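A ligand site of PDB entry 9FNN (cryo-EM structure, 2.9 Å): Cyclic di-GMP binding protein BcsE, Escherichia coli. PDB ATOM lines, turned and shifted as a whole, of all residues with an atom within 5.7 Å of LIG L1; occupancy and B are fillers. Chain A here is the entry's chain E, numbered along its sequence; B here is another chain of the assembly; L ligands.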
ATOM      1  N   ALA A 316       3.931 -17.362 -31.387  1.00  0.00           N
ATOM      2  CA  ALA A 316       3.879 -18.778 -31.025  1.00  0.00           C
ATOM      3  C   ALA A 316       2.618 -19.388 -31.625  1.00  0.00           C
ATOM      4  O   ALA A 316       1.576 -19.539 -30.983  1.00  0.00           O
ATOM      5  CB  ALA A 316       3.913 -18.950 -29.510  1.00  0.00           C
ATOM      6  N   LEU A 318       2.759 -22.438 -33.814  1.00  0.00           N
ATOM      7  CA  LEU A 318       3.332 -23.570 -34.532  1.00  0.00           C
ATOM      8  C   LEU A 318       3.548 -24.727 -33.558  1.00  0.00           C
ATOM      9  O   LEU A 318       3.923 -24.515 -32.409  1.00  0.00           O
ATOM     10  CB  LEU A 318       4.655 -23.177 -35.196  1.00  0.00           C
ATOM     11  CG  LEU A 318       5.246 -24.079 -36.273  1.00  0.00           C
ATOM     12  CD1 LEU A 318       4.395 -24.016 -37.516  1.00  0.00           C
ATOM     13  CD2 LEU A 318       6.662 -23.664 -36.574  1.00  0.00           C
ATOM     14  N   ARG A 319       3.318 -25.947 -34.048  1.00  0.00           N
ATOM     15  CA  ARG A 319       3.623 -27.165 -33.323  1.00  0.00           C
ATOM     16  C   ARG A 319       4.799 -27.873 -33.974  1.00  0.00           C
ATOM     17  O   ARG A 319       5.240 -27.511 -35.074  1.00  0.00           O
ATOM     18  CB  ARG A 319       2.412 -28.103 -33.285  1.00  0.00           C
ATOM     19  CG  ARG A 319       1.268 -27.610 -32.430  1.00  0.00           C
ATOM     20  CD  ARG A 319       0.169 -28.647 -32.384  1.00  0.00           C
ATOM     21  NE  ARG A 319      -0.999 -28.176 -31.665  1.00  0.00           N
ATOM     22  CZ  ARG A 319      -2.134 -28.860 -31.557  1.00  0.00           C
ATOM     23  NH1 ARG A 319      -2.277 -30.043 -32.111  1.00  0.00           N
ATOM     24  NH2 ARG A 319      -3.144 -28.326 -30.880  1.00  0.00           N
ATOM     25  N   ALA A 320       5.324 -28.884 -33.287  1.00  0.00           N
ATOM     26  CA  ALA A 320       6.417 -29.669 -33.842  1.00  0.00           C
ATOM     27  C   ALA A 320       5.978 -30.389 -35.107  1.00  0.00           C
ATOM     28  O   ALA A 320       6.739 -30.473 -36.082  1.00  0.00           O
ATOM     29  CB  ALA A 320       6.934 -30.665 -32.801  1.00  0.00           C
ATOM     30  N   THR A 321       4.751 -30.919 -35.116  1.00  0.00           N
ATOM     31  CA  THR A 321       4.249 -31.610 -36.296  1.00  0.00           C
ATOM     32  C   THR A 321       4.139 -30.659 -37.488  1.00  0.00           C
ATOM     33  O   THR A 321       4.473 -31.039 -38.618  1.00  0.00           O
ATOM     34  CB  THR A 321       2.887 -32.226 -35.978  1.00  0.00           C
ATOM     35  OG1 THR A 321       1.907 -31.194 -35.857  1.00  0.00           O
ATOM     36  CG2 THR A 321       2.955 -32.988 -34.671  1.00  0.00           C
ATOM     37  N   ASN A 427      -7.054 -32.522 -23.927  1.00  0.00           N
ATOM     38  CA  ASN A 427      -7.514 -31.392 -24.721  1.00  0.00           C
ATOM     39  C   ASN A 427      -7.326 -31.583 -26.212  1.00  0.00           C
ATOM     40  O   ASN A 427      -8.125 -31.053 -26.988  1.00  0.00           O
ATOM     41  CB  ASN A 427      -6.783 -30.114 -24.300  1.00  0.00           C
ATOM     42  CG  ASN A 427      -7.129 -29.696 -22.885  1.00  0.00           C
ATOM     43  OD1 ASN A 427      -8.256 -29.898 -22.421  1.00  0.00           O
ATOM     44  ND2 ASN A 427      -6.166 -29.105 -22.189  1.00  0.00           N
ATOM     45  N   ARG A 428      -6.305 -32.319 -26.647  1.00  0.00           N
ATOM     46  CA  ARG A 428      -6.051 -32.501 -28.063  1.00  0.00           C
ATOM     47  C   ARG A 428      -6.829 -33.696 -28.596  1.00  0.00           C
ATOM     48  O   ARG A 428      -7.414 -34.478 -27.852  1.00  0.00           O
ATOM     49  CB  ARG A 428      -4.553 -32.675 -28.324  1.00  0.00           C
ATOM     50  CG  ARG A 428      -3.733 -31.431 -28.120  1.00  0.00           C
ATOM     51  CD  ARG A 428      -2.341 -31.634 -28.695  1.00  0.00           C
ATOM     52  NE  ARG A 428      -1.476 -30.475 -28.492  1.00  0.00           N
ATOM     53  CZ  ARG A 428      -0.229 -30.390 -28.939  1.00  0.00           C
ATOM     54  NH1 ARG A 428       0.314 -31.371 -29.635  1.00  0.00           N
ATOM     55  NH2 ARG A 428       0.477 -29.294 -28.693  1.00  0.00           N
ATOM     56  N   ASP A 431      -5.067 -37.560 -28.028  1.00  0.00           N
ATOM     57  CA  ASP A 431      -4.797 -38.041 -26.685  1.00  0.00           C
ATOM     58  C   ASP A 431      -5.911 -38.980 -26.239  1.00  0.00           C
ATOM     59  O   ASP A 431      -7.085 -38.622 -26.297  1.00  0.00           O
ATOM     60  CB  ASP A 431      -4.678 -36.870 -25.707  1.00  0.00           C
ATOM     61  CG  ASP A 431      -3.567 -35.916 -26.082  1.00  0.00           C
ATOM     62  OD1 ASP A 431      -2.842 -36.190 -27.058  1.00  0.00           O
ATOM     63  OD2 ASP A 431      -3.431 -34.868 -25.400  1.00  0.00           O
ATOM     64  N   LEU A 444      -0.156 -39.844 -25.447  1.00  0.00           N
ATOM     65  CA  LEU A 444      -0.161 -38.475 -25.931  1.00  0.00           C
ATOM     66  C   LEU A 444       0.479 -38.458 -27.322  1.00  0.00           C
ATOM     67  O   LEU A 444       1.655 -38.806 -27.462  1.00  0.00           O
ATOM     68  CB  LEU A 444       0.592 -37.552 -24.971  1.00  0.00           C
ATOM     69  CG  LEU A 444       0.139 -37.695 -23.523  1.00  0.00           C
ATOM     70  CD1 LEU A 444       0.918 -36.754 -22.629  1.00  0.00           C
ATOM     71  CD2 LEU A 444      -1.343 -37.431 -23.411  1.00  0.00           C
ATOM     72  N   SER A 445      -0.287 -38.047 -28.317  1.00  0.00           N
ATOM     73  CA  SER A 445       0.185 -38.115 -29.688  1.00  0.00           C
ATOM     74  C   SER A 445       1.210 -37.022 -29.945  1.00  0.00           C
ATOM     75  O   SER A 445       0.957 -35.844 -29.677  1.00  0.00           O
ATOM     76  CB  SER A 445      -0.987 -37.990 -30.663  1.00  0.00           C
ATOM     77  OG  SER A 445      -0.560 -38.095 -32.004  1.00  0.00           O
ATOM     78  N   PHE A 446       2.372 -37.417 -30.457  1.00  0.00           N
ATOM     79  CA  PHE A 446       3.460 -36.547 -30.889  1.00  0.00           C
ATOM     80  C   PHE A 446       4.091 -35.764 -29.745  1.00  0.00           C
ATOM     81  O   PHE A 446       4.956 -34.914 -30.000  1.00  0.00           O
ATOM     82  CB  PHE A 446       2.993 -35.583 -31.980  1.00  0.00           C
ATOM     83  CG  PHE A 446       2.577 -36.269 -33.241  1.00  0.00           C
ATOM     84  CD1 PHE A 446       3.400 -37.195 -33.838  1.00  0.00           C
ATOM     85  CD2 PHE A 446       1.354 -35.998 -33.818  1.00  0.00           C
ATOM     86  CE1 PHE A 446       3.032 -37.828 -34.990  1.00  0.00           C
ATOM     87  CE2 PHE A 446       0.976 -36.631 -34.971  1.00  0.00           C
ATOM     88  CZ  PHE A 446       1.809 -37.552 -35.559  1.00  0.00           C
ATOM     89  N   CYS A 447       3.701 -36.024 -28.505  1.00  0.00           N
ATOM     90  CA  CYS A 447       4.389 -35.425 -27.376  1.00  0.00           C
ATOM     91  C   CYS A 447       5.781 -36.028 -27.243  1.00  0.00           C
ATOM     92  O   CYS A 447       5.978 -37.227 -27.433  1.00  0.00           O
ATOM     93  CB  CYS A 447       3.587 -35.651 -26.092  1.00  0.00           C
ATOM     94  SG  CYS A 447       4.445 -35.193 -24.592  1.00  0.00           S
ATOM     95  N   ARG A 448       6.755 -35.185 -26.928  1.00  0.00           N
ATOM     96  CA  ARG A 448       8.110 -35.661 -26.692  1.00  0.00           C
ATOM     97  C   ARG A 448       8.318 -35.937 -25.210  1.00  0.00           C
ATOM     98  O   ARG A 448       7.619 -35.407 -24.346  1.00  0.00           O
ATOM     99  CB  ARG A 448       9.143 -34.659 -27.207  1.00  0.00           C
ATOM    100  CG  ARG A 448       9.629 -34.953 -28.617  1.00  0.00           C
ATOM    101  CD  ARG A 448      10.954 -34.284 -28.906  1.00  0.00           C
ATOM    102  NE  ARG A 448      10.789 -32.939 -29.448  1.00  0.00           N
ATOM    103  CZ  ARG A 448      10.894 -32.626 -30.731  1.00  0.00           C
ATOM    104  NH1 ARG A 448      11.173 -33.545 -31.644  1.00  0.00           N
ATOM    105  NH2 ARG A 448      10.714 -31.367 -31.114  1.00  0.00           N
ATOM    106  N   ASP A 451       8.952 -32.916 -22.894  1.00  0.00           N
ATOM    107  CA  ASP A 451       7.757 -32.102 -22.650  1.00  0.00           C
ATOM    108  C   ASP A 451       6.554 -32.950 -22.264  1.00  0.00           C
ATOM    109  O   ASP A 451       5.470 -32.819 -22.822  1.00  0.00           O
ATOM    110  CB  ASP A 451       7.461 -31.253 -23.881  1.00  0.00           C
ATOM    111  CG  ASP A 451       8.513 -30.189 -24.123  1.00  0.00           C
ATOM    112  OD1 ASP A 451       9.137 -29.740 -23.141  1.00  0.00           O
ATOM    113  OD2 ASP A 451       8.708 -29.805 -25.295  1.00  0.00           O
ATOM    114  N   THR A 454       4.616 -30.940 -18.861  1.00  0.00           N
ATOM    115  CA  THR A 454       3.742 -29.846 -19.292  1.00  0.00           C
ATOM    116  C   THR A 454       2.411 -30.381 -19.785  1.00  0.00           C
ATOM    117  O   THR A 454       1.337 -29.862 -19.428  1.00  0.00           O
ATOM    118  CB  THR A 454       4.430 -29.028 -20.380  1.00  0.00           C
ATOM    119  OG1 THR A 454       4.544 -29.814 -21.570  1.00  0.00           O
ATOM    120  CG2 THR A 454       5.815 -28.606 -19.940  1.00  0.00           C
ATOM    121  N   ALA A 455       2.443 -31.440 -20.605  1.00  0.00           N
ATOM    122  CA  ALA A 455       1.207 -32.036 -21.088  1.00  0.00           C
ATOM    123  C   ALA A 455       0.376 -32.595 -19.945  1.00  0.00           C
ATOM    124  O   ALA A 455      -0.847 -32.406 -19.903  1.00  0.00           O
ATOM    125  CB  ALA A 455       1.527 -33.140 -22.107  1.00  0.00           C
ATOM    126  N   HIS A 458      -1.305 -29.836 -18.110  1.00  0.00           N
ATOM    127  CA  HIS A 458      -2.496 -29.405 -18.851  1.00  0.00           C
ATOM    128  C   HIS A 458      -3.659 -30.361 -18.622  1.00  0.00           C
ATOM    129  O   HIS A 458      -4.800 -29.925 -18.437  1.00  0.00           O
ATOM    130  CB  HIS A 458      -2.174 -29.292 -20.341  1.00  0.00           C
ATOM    131  CG  HIS A 458      -1.206 -28.205 -20.664  1.00  0.00           C
ATOM    132  ND1 HIS A 458      -0.496 -28.176 -21.845  1.00  0.00           N
ATOM    133  CD2 HIS A 458      -0.826 -27.109 -19.970  1.00  0.00           C
ATOM    134  CE1 HIS A 458       0.283 -27.113 -21.864  1.00  0.00           C
ATOM    135  NE2 HIS A 458       0.103 -26.444 -20.738  1.00  0.00           N
ATOM    136  N   ILE A 459      -3.381 -31.667 -18.631  1.00  0.00           N
ATOM    137  CA  ILE A 459      -4.458 -32.652 -18.544  1.00  0.00           C
ATOM    138  C   ILE A 459      -5.088 -32.674 -17.162  1.00  0.00           C
ATOM    139  O   ILE A 459      -6.312 -32.667 -17.012  1.00  0.00           O
ATOM    140  CB  ILE A 459      -3.943 -34.042 -18.946  1.00  0.00           C
ATOM    141  CG1 ILE A 459      -3.571 -34.060 -20.436  1.00  0.00           C
ATOM    142  CG2 ILE A 459      -4.977 -35.107 -18.659  1.00  0.00           C
ATOM    143  CD1 ILE A 459      -3.027 -35.382 -20.896  1.00  0.00           C
ATOM    144  N   SER B 342      13.013 -28.279 -27.206  1.00  0.00           N
ATOM    145  CA  SER B 342      12.186 -28.909 -28.230  1.00  0.00           C
ATOM    146  C   SER B 342      12.441 -28.296 -29.601  1.00  0.00           C
ATOM    147  O   SER B 342      12.569 -29.016 -30.599  1.00  0.00           O
ATOM    148  CB  SER B 342      10.709 -28.779 -27.855  1.00  0.00           C
ATOM    149  OG  SER B 342      10.462 -29.373 -26.595  1.00  0.00           O
HETATM  150  P1  LIG L   1       4.311 -28.327 -29.434  1.00  0.00           P
HETATM  151  O1  LIG L   1       3.139 -29.135 -29.917  1.00  0.00           O
HETATM  152  O2  LIG L   1       5.343 -27.931 -30.454  1.00  0.00           O
HETATM  153  O3  LIG L   1       3.772 -27.009 -28.700  1.00  0.00           O
HETATM  154  C1  LIG L   1       4.558 -25.791 -28.812  1.00  0.00           C
HETATM  155  C2  LIG L   1       3.787 -24.615 -28.266  1.00  0.00           C
HETATM  156  O4  LIG L   1       2.777 -24.215 -29.225  1.00  0.00           O
HETATM  157  C3  LIG L   1       3.033 -24.862 -26.970  1.00  0.00           C
HETATM  158  O5  LIG L   1       3.899 -24.695 -25.848  1.00  0.00           O
HETATM  159  C4  LIG L   1       1.947 -23.785 -27.044  1.00  0.00           C
HETATM  160  O6  LIG L   1       2.360 -22.530 -26.536  1.00  0.00           O
HETATM  161  C5  LIG L   1       1.656 -23.691 -28.544  1.00  0.00           C
HETATM  162  N1  LIG L   1       0.466 -24.420 -28.967  1.00  0.00           N
HETATM  163  C6  LIG L   1       0.427 -25.562 -29.723  1.00  0.00           C
HETATM  164  N2  LIG L   1      -0.789 -25.985 -29.957  1.00  0.00           N
HETATM  165  C7  LIG L   1      -1.605 -25.064 -29.323  1.00  0.00           C
HETATM  166  C8  LIG L   1      -3.022 -25.011 -29.234  1.00  0.00           C
HETATM  167  O7  LIG L   1      -3.851 -25.789 -29.717  1.00  0.00           O
HETATM  168  N3  LIG L   1      -3.439 -23.914 -28.484  1.00  0.00           N
HETATM  169  C9  LIG L   1      -2.604 -22.983 -27.901  1.00  0.00           C
HETATM  170  N4  LIG L   1      -3.206 -21.993 -27.221  1.00  0.00           N
HETATM  171  N5  LIG L   1      -1.277 -23.032 -27.981  1.00  0.00           N
HETATM  172  C10 LIG L   1      -0.849 -24.094 -28.704  1.00  0.00           C
HETATM  173  P2  LIG L   1       3.629 -25.760 -24.669  1.00  0.00           P
HETATM  174  O8  LIG L   1       2.213 -25.669 -24.182  1.00  0.00           O
HETATM  175  O9  LIG L   1       4.709 -25.603 -23.629  1.00  0.00           O
HETATM  176  O10 LIG L   1       3.830 -27.163 -25.419  1.00  0.00           O
HETATM  177  C11 LIG L   1       5.119 -27.817 -25.317  1.00  0.00           C
HETATM  178  C12 LIG L   1       5.007 -29.226 -25.841  1.00  0.00           C
HETATM  179  O11 LIG L   1       4.295 -30.049 -24.875  1.00  0.00           O
HETATM  180  C13 LIG L   1       4.221 -29.390 -27.134  1.00  0.00           C
HETATM  181  O12 LIG L   1       5.067 -29.124 -28.246  1.00  0.00           O
HETATM  182  C14 LIG L   1       3.789 -30.847 -27.038  1.00  0.00           C
HETATM  183  O13 LIG L   1       4.792 -31.770 -27.420  1.00  0.00           O
HETATM  184  C15 LIG L   1       3.485 -30.984 -25.546  1.00  0.00           C
HETATM  185  N6  LIG L   1       2.080 -30.726 -25.215  1.00  0.00           N
HETATM  186  C16 LIG L   1       1.562 -29.609 -24.601  1.00  0.00           C
HETATM  187  N7  LIG L   1       0.273 -29.669 -24.440  1.00  0.00           N
HETATM  188  C17 LIG L   1      -0.087 -30.901 -24.959  1.00  0.00           C
HETATM  189  C18 LIG L   1      -1.367 -31.519 -25.058  1.00  0.00           C
HETATM  190  O14 LIG L   1      -2.458 -31.074 -24.674  1.00  0.00           O
HETATM  191  N8  LIG L   1      -1.282 -32.771 -25.652  1.00  0.00           N
HETATM  192  C19 LIG L   1      -0.127 -33.357 -26.119  1.00  0.00           C
HETATM  193  N9  LIG L   1      -0.243 -34.565 -26.670  1.00  0.00           N
HETATM  194  N10 LIG L   1       1.079 -32.783 -26.032  1.00  0.00           N
HETATM  195  C20 LIG L   1       1.022 -31.560 -25.445  1.00  0.00           C
HETATM  196  P1  LG2 L   2      -7.488 -23.661 -29.203  1.00  0.00           P
HETATM  197  O1  LG2 L   2      -6.204 -22.903 -28.986  1.00  0.00           O
HETATM  198  O2  LG2 L   2      -8.701 -22.857 -29.564  1.00  0.00           O
HETATM  199  O3  LG2 L   2      -7.241 -24.761 -30.338  1.00  0.00           O
HETATM  200  C1  LG2 L   2      -8.357 -25.203 -31.149  1.00  0.00           C
HETATM  201  C2  LG2 L   2      -7.842 -26.073 -32.266  1.00  0.00           C
HETATM  202  O4  LG2 L   2      -7.053 -25.247 -33.166  1.00  0.00           O
HETATM  203  C3  LG2 L   2      -6.900 -27.190 -31.823  1.00  0.00           C
HETATM  204  O5  LG2 L   2      -7.652 -28.349 -31.505  1.00  0.00           O
HETATM  205  C4  LG2 L   2      -6.013 -27.379 -33.057  1.00  0.00           C
HETATM  206  O6  LG2 L   2      -6.561 -28.246 -34.020  1.00  0.00           O
HETATM  207  C5  LG2 L   2      -5.920 -25.956 -33.613  1.00  0.00           C
HETATM  208  N1  LG2 L   2      -4.709 -25.238 -33.229  1.00  0.00           N
HETATM  209  C6  LG2 L   2      -4.602 -24.115 -32.452  1.00  0.00           C
HETATM  210  N2  LG2 L   2      -3.371 -23.695 -32.307  1.00  0.00           N
HETATM  211  C7  LG2 L   2      -2.618 -24.599 -33.052  1.00  0.00           C
HETATM  212  C8  LG2 L   2      -1.214 -24.653 -33.276  1.00  0.00           C
HETATM  213  O7  LG2 L   2      -0.343 -23.890 -32.853  1.00  0.00           O
HETATM  214  N3  LG2 L   2      -0.880 -25.719 -34.112  1.00  0.00           N
HETATM  215  C9  LG2 L   2      -1.767 -26.627 -34.640  1.00  0.00           C
HETATM  216  N4  LG2 L   2      -1.259 -27.598 -35.410  1.00  0.00           N
HETATM  217  N5  LG2 L   2      -3.082 -26.585 -34.420  1.00  0.00           N
HETATM  218  C10 LG2 L   2      -3.426 -25.551 -33.624  1.00  0.00           C
HETATM  219  P2  LG2 L   2      -7.044 -29.200 -30.279  1.00  0.00           P
HETATM  220  O8  LG2 L   2      -5.701 -29.755 -30.647  1.00  0.00           O
HETATM  221  O9  LG2 L   2      -8.100 -30.184 -29.842  1.00  0.00           O
HETATM  222  O10 LG2 L   2      -6.847 -28.077 -29.139  1.00  0.00           O
HETATM  223  C11 LG2 L   2      -7.950 -27.797 -28.227  1.00  0.00           C
HETATM  224  C12 LG2 L   2      -7.481 -26.845 -27.163  1.00  0.00           C
HETATM  225  O11 LG2 L   2      -6.450 -27.483 -26.372  1.00  0.00           O
HETATM  226  C13 LG2 L   2      -6.839 -25.555 -27.664  1.00  0.00           C
HETATM  227  O12 LG2 L   2      -7.841 -24.565 -27.929  1.00  0.00           O
HETATM  228  C14 LG2 L   2      -5.949 -25.165 -26.479  1.00  0.00           C
HETATM  229  O13 LG2 L   2      -6.606 -24.402 -25.488  1.00  0.00           O
HETATM  230  C15 LG2 L   2      -5.514 -26.522 -25.927  1.00  0.00           C
HETATM  231  N6  LG2 L   2      -4.178 -26.937 -26.335  1.00  0.00           N
HETATM  232  C16 LG2 L   2      -3.850 -27.953 -27.185  1.00  0.00           C
HETATM  233  N7  LG2 L   2      -2.556 -28.092 -27.355  1.00  0.00           N
HETATM  234  C17 LG2 L   2      -1.999 -27.094 -26.551  1.00  0.00           C
HETATM  235  C18 LG2 L   2      -0.648 -26.763 -26.334  1.00  0.00           C
HETATM  236  O14 LG2 L   2       0.370 -27.289 -26.801  1.00  0.00           O
HETATM  237  N8  LG2 L   2      -0.532 -25.688 -25.452  1.00  0.00           N
HETATM  238  C19 LG2 L   2      -1.577 -25.023 -24.856  1.00  0.00           C
HETATM  239  N9  LG2 L   2      -1.261 -24.014 -24.038  1.00  0.00           N
HETATM  240  N10 LG2 L   2      -2.857 -25.341 -25.056  1.00  0.00           N
HETATM  241  C20 LG2 L   2      -2.992 -26.383 -25.921  1.00  0.00           C
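An oxygen (O4) of LIG L1 sits close to the backbone carbonyl oxygen of Leu 318 (3.4 Å). Residues that only touch LIG L1: Leu 444, Cys 447, Arg 448, Asp 451 and Ala 455. Hydrophobic or aromatic side chains that line LIG L1: Ala 320, Leu 444, Ala 455 and His 458. The nearest printed residue that does not touch LIG L1 is Phe 446 (4.1 Å).
An oxygen (O1) of LG2 L2 sits at hydrogen-bond distance from a nitrogen (N3) of LIG L1 (3.0 Å).
The guanidinium group (NE) of Arg 319 is in hydrogen-bond range of a nitrogen (N2) of LIG L1 (2.8 Å). The guanidinium group (NH2) of Arg 428 is in salt-bridge range of an oxygen (O1) of LIG L1. N of Ala 320 is in hydrogen-bond range of O2 of LIG L1. OD2 of Asp 431 sits at hydrogen-bond distance from N8 of LIG L1 (3.0 Å). ND1 of His 458 lies within hydrogen-bond range of N7 of LIG L1, at 3.1 Å. An oxygen (O11) of LIG L1 sits at hydrogen-bond distance from the side-chain hydroxyl of Thr 454, 3.3 Å away. O of Ser 445 sits at hydrogen-bond distance from N9 of LIG L1 (3.5 Å). An oxygen (O8) of LG2 L2 lies within salt-bridge range of the guanidinium group (NH2) of Arg 319 (2.9 Å). An oxygen (O14) of LG2 L2 lies within hydrogen-bond range of the guanidinium group of Arg 428 (2.8 Å). The backbone carbonyl oxygen of Asn 427 sits close to an oxygen (O9) of LG2 L2.
The side-chain carboxylate (OD1) of Asp 431 is in hydrogen-bond range of the backbone NH (N) of Ser 445. O of Thr 454 sits close to ND1 of His 458, 3.5 Å away. OG1 of Thr 454 is in hydrogen-bond range of O of Asp 451, at 3.4 Å. The backbone carbonyl oxygen (O) of Asp 451 lies within hydrogen-bond range of the side-chain sulfur (SG) of Cys 447 (3.1 Å). O of Ser 342 of chain B is in hydrogen-bond range of NH2 of Arg 448, at 3.0 Å.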
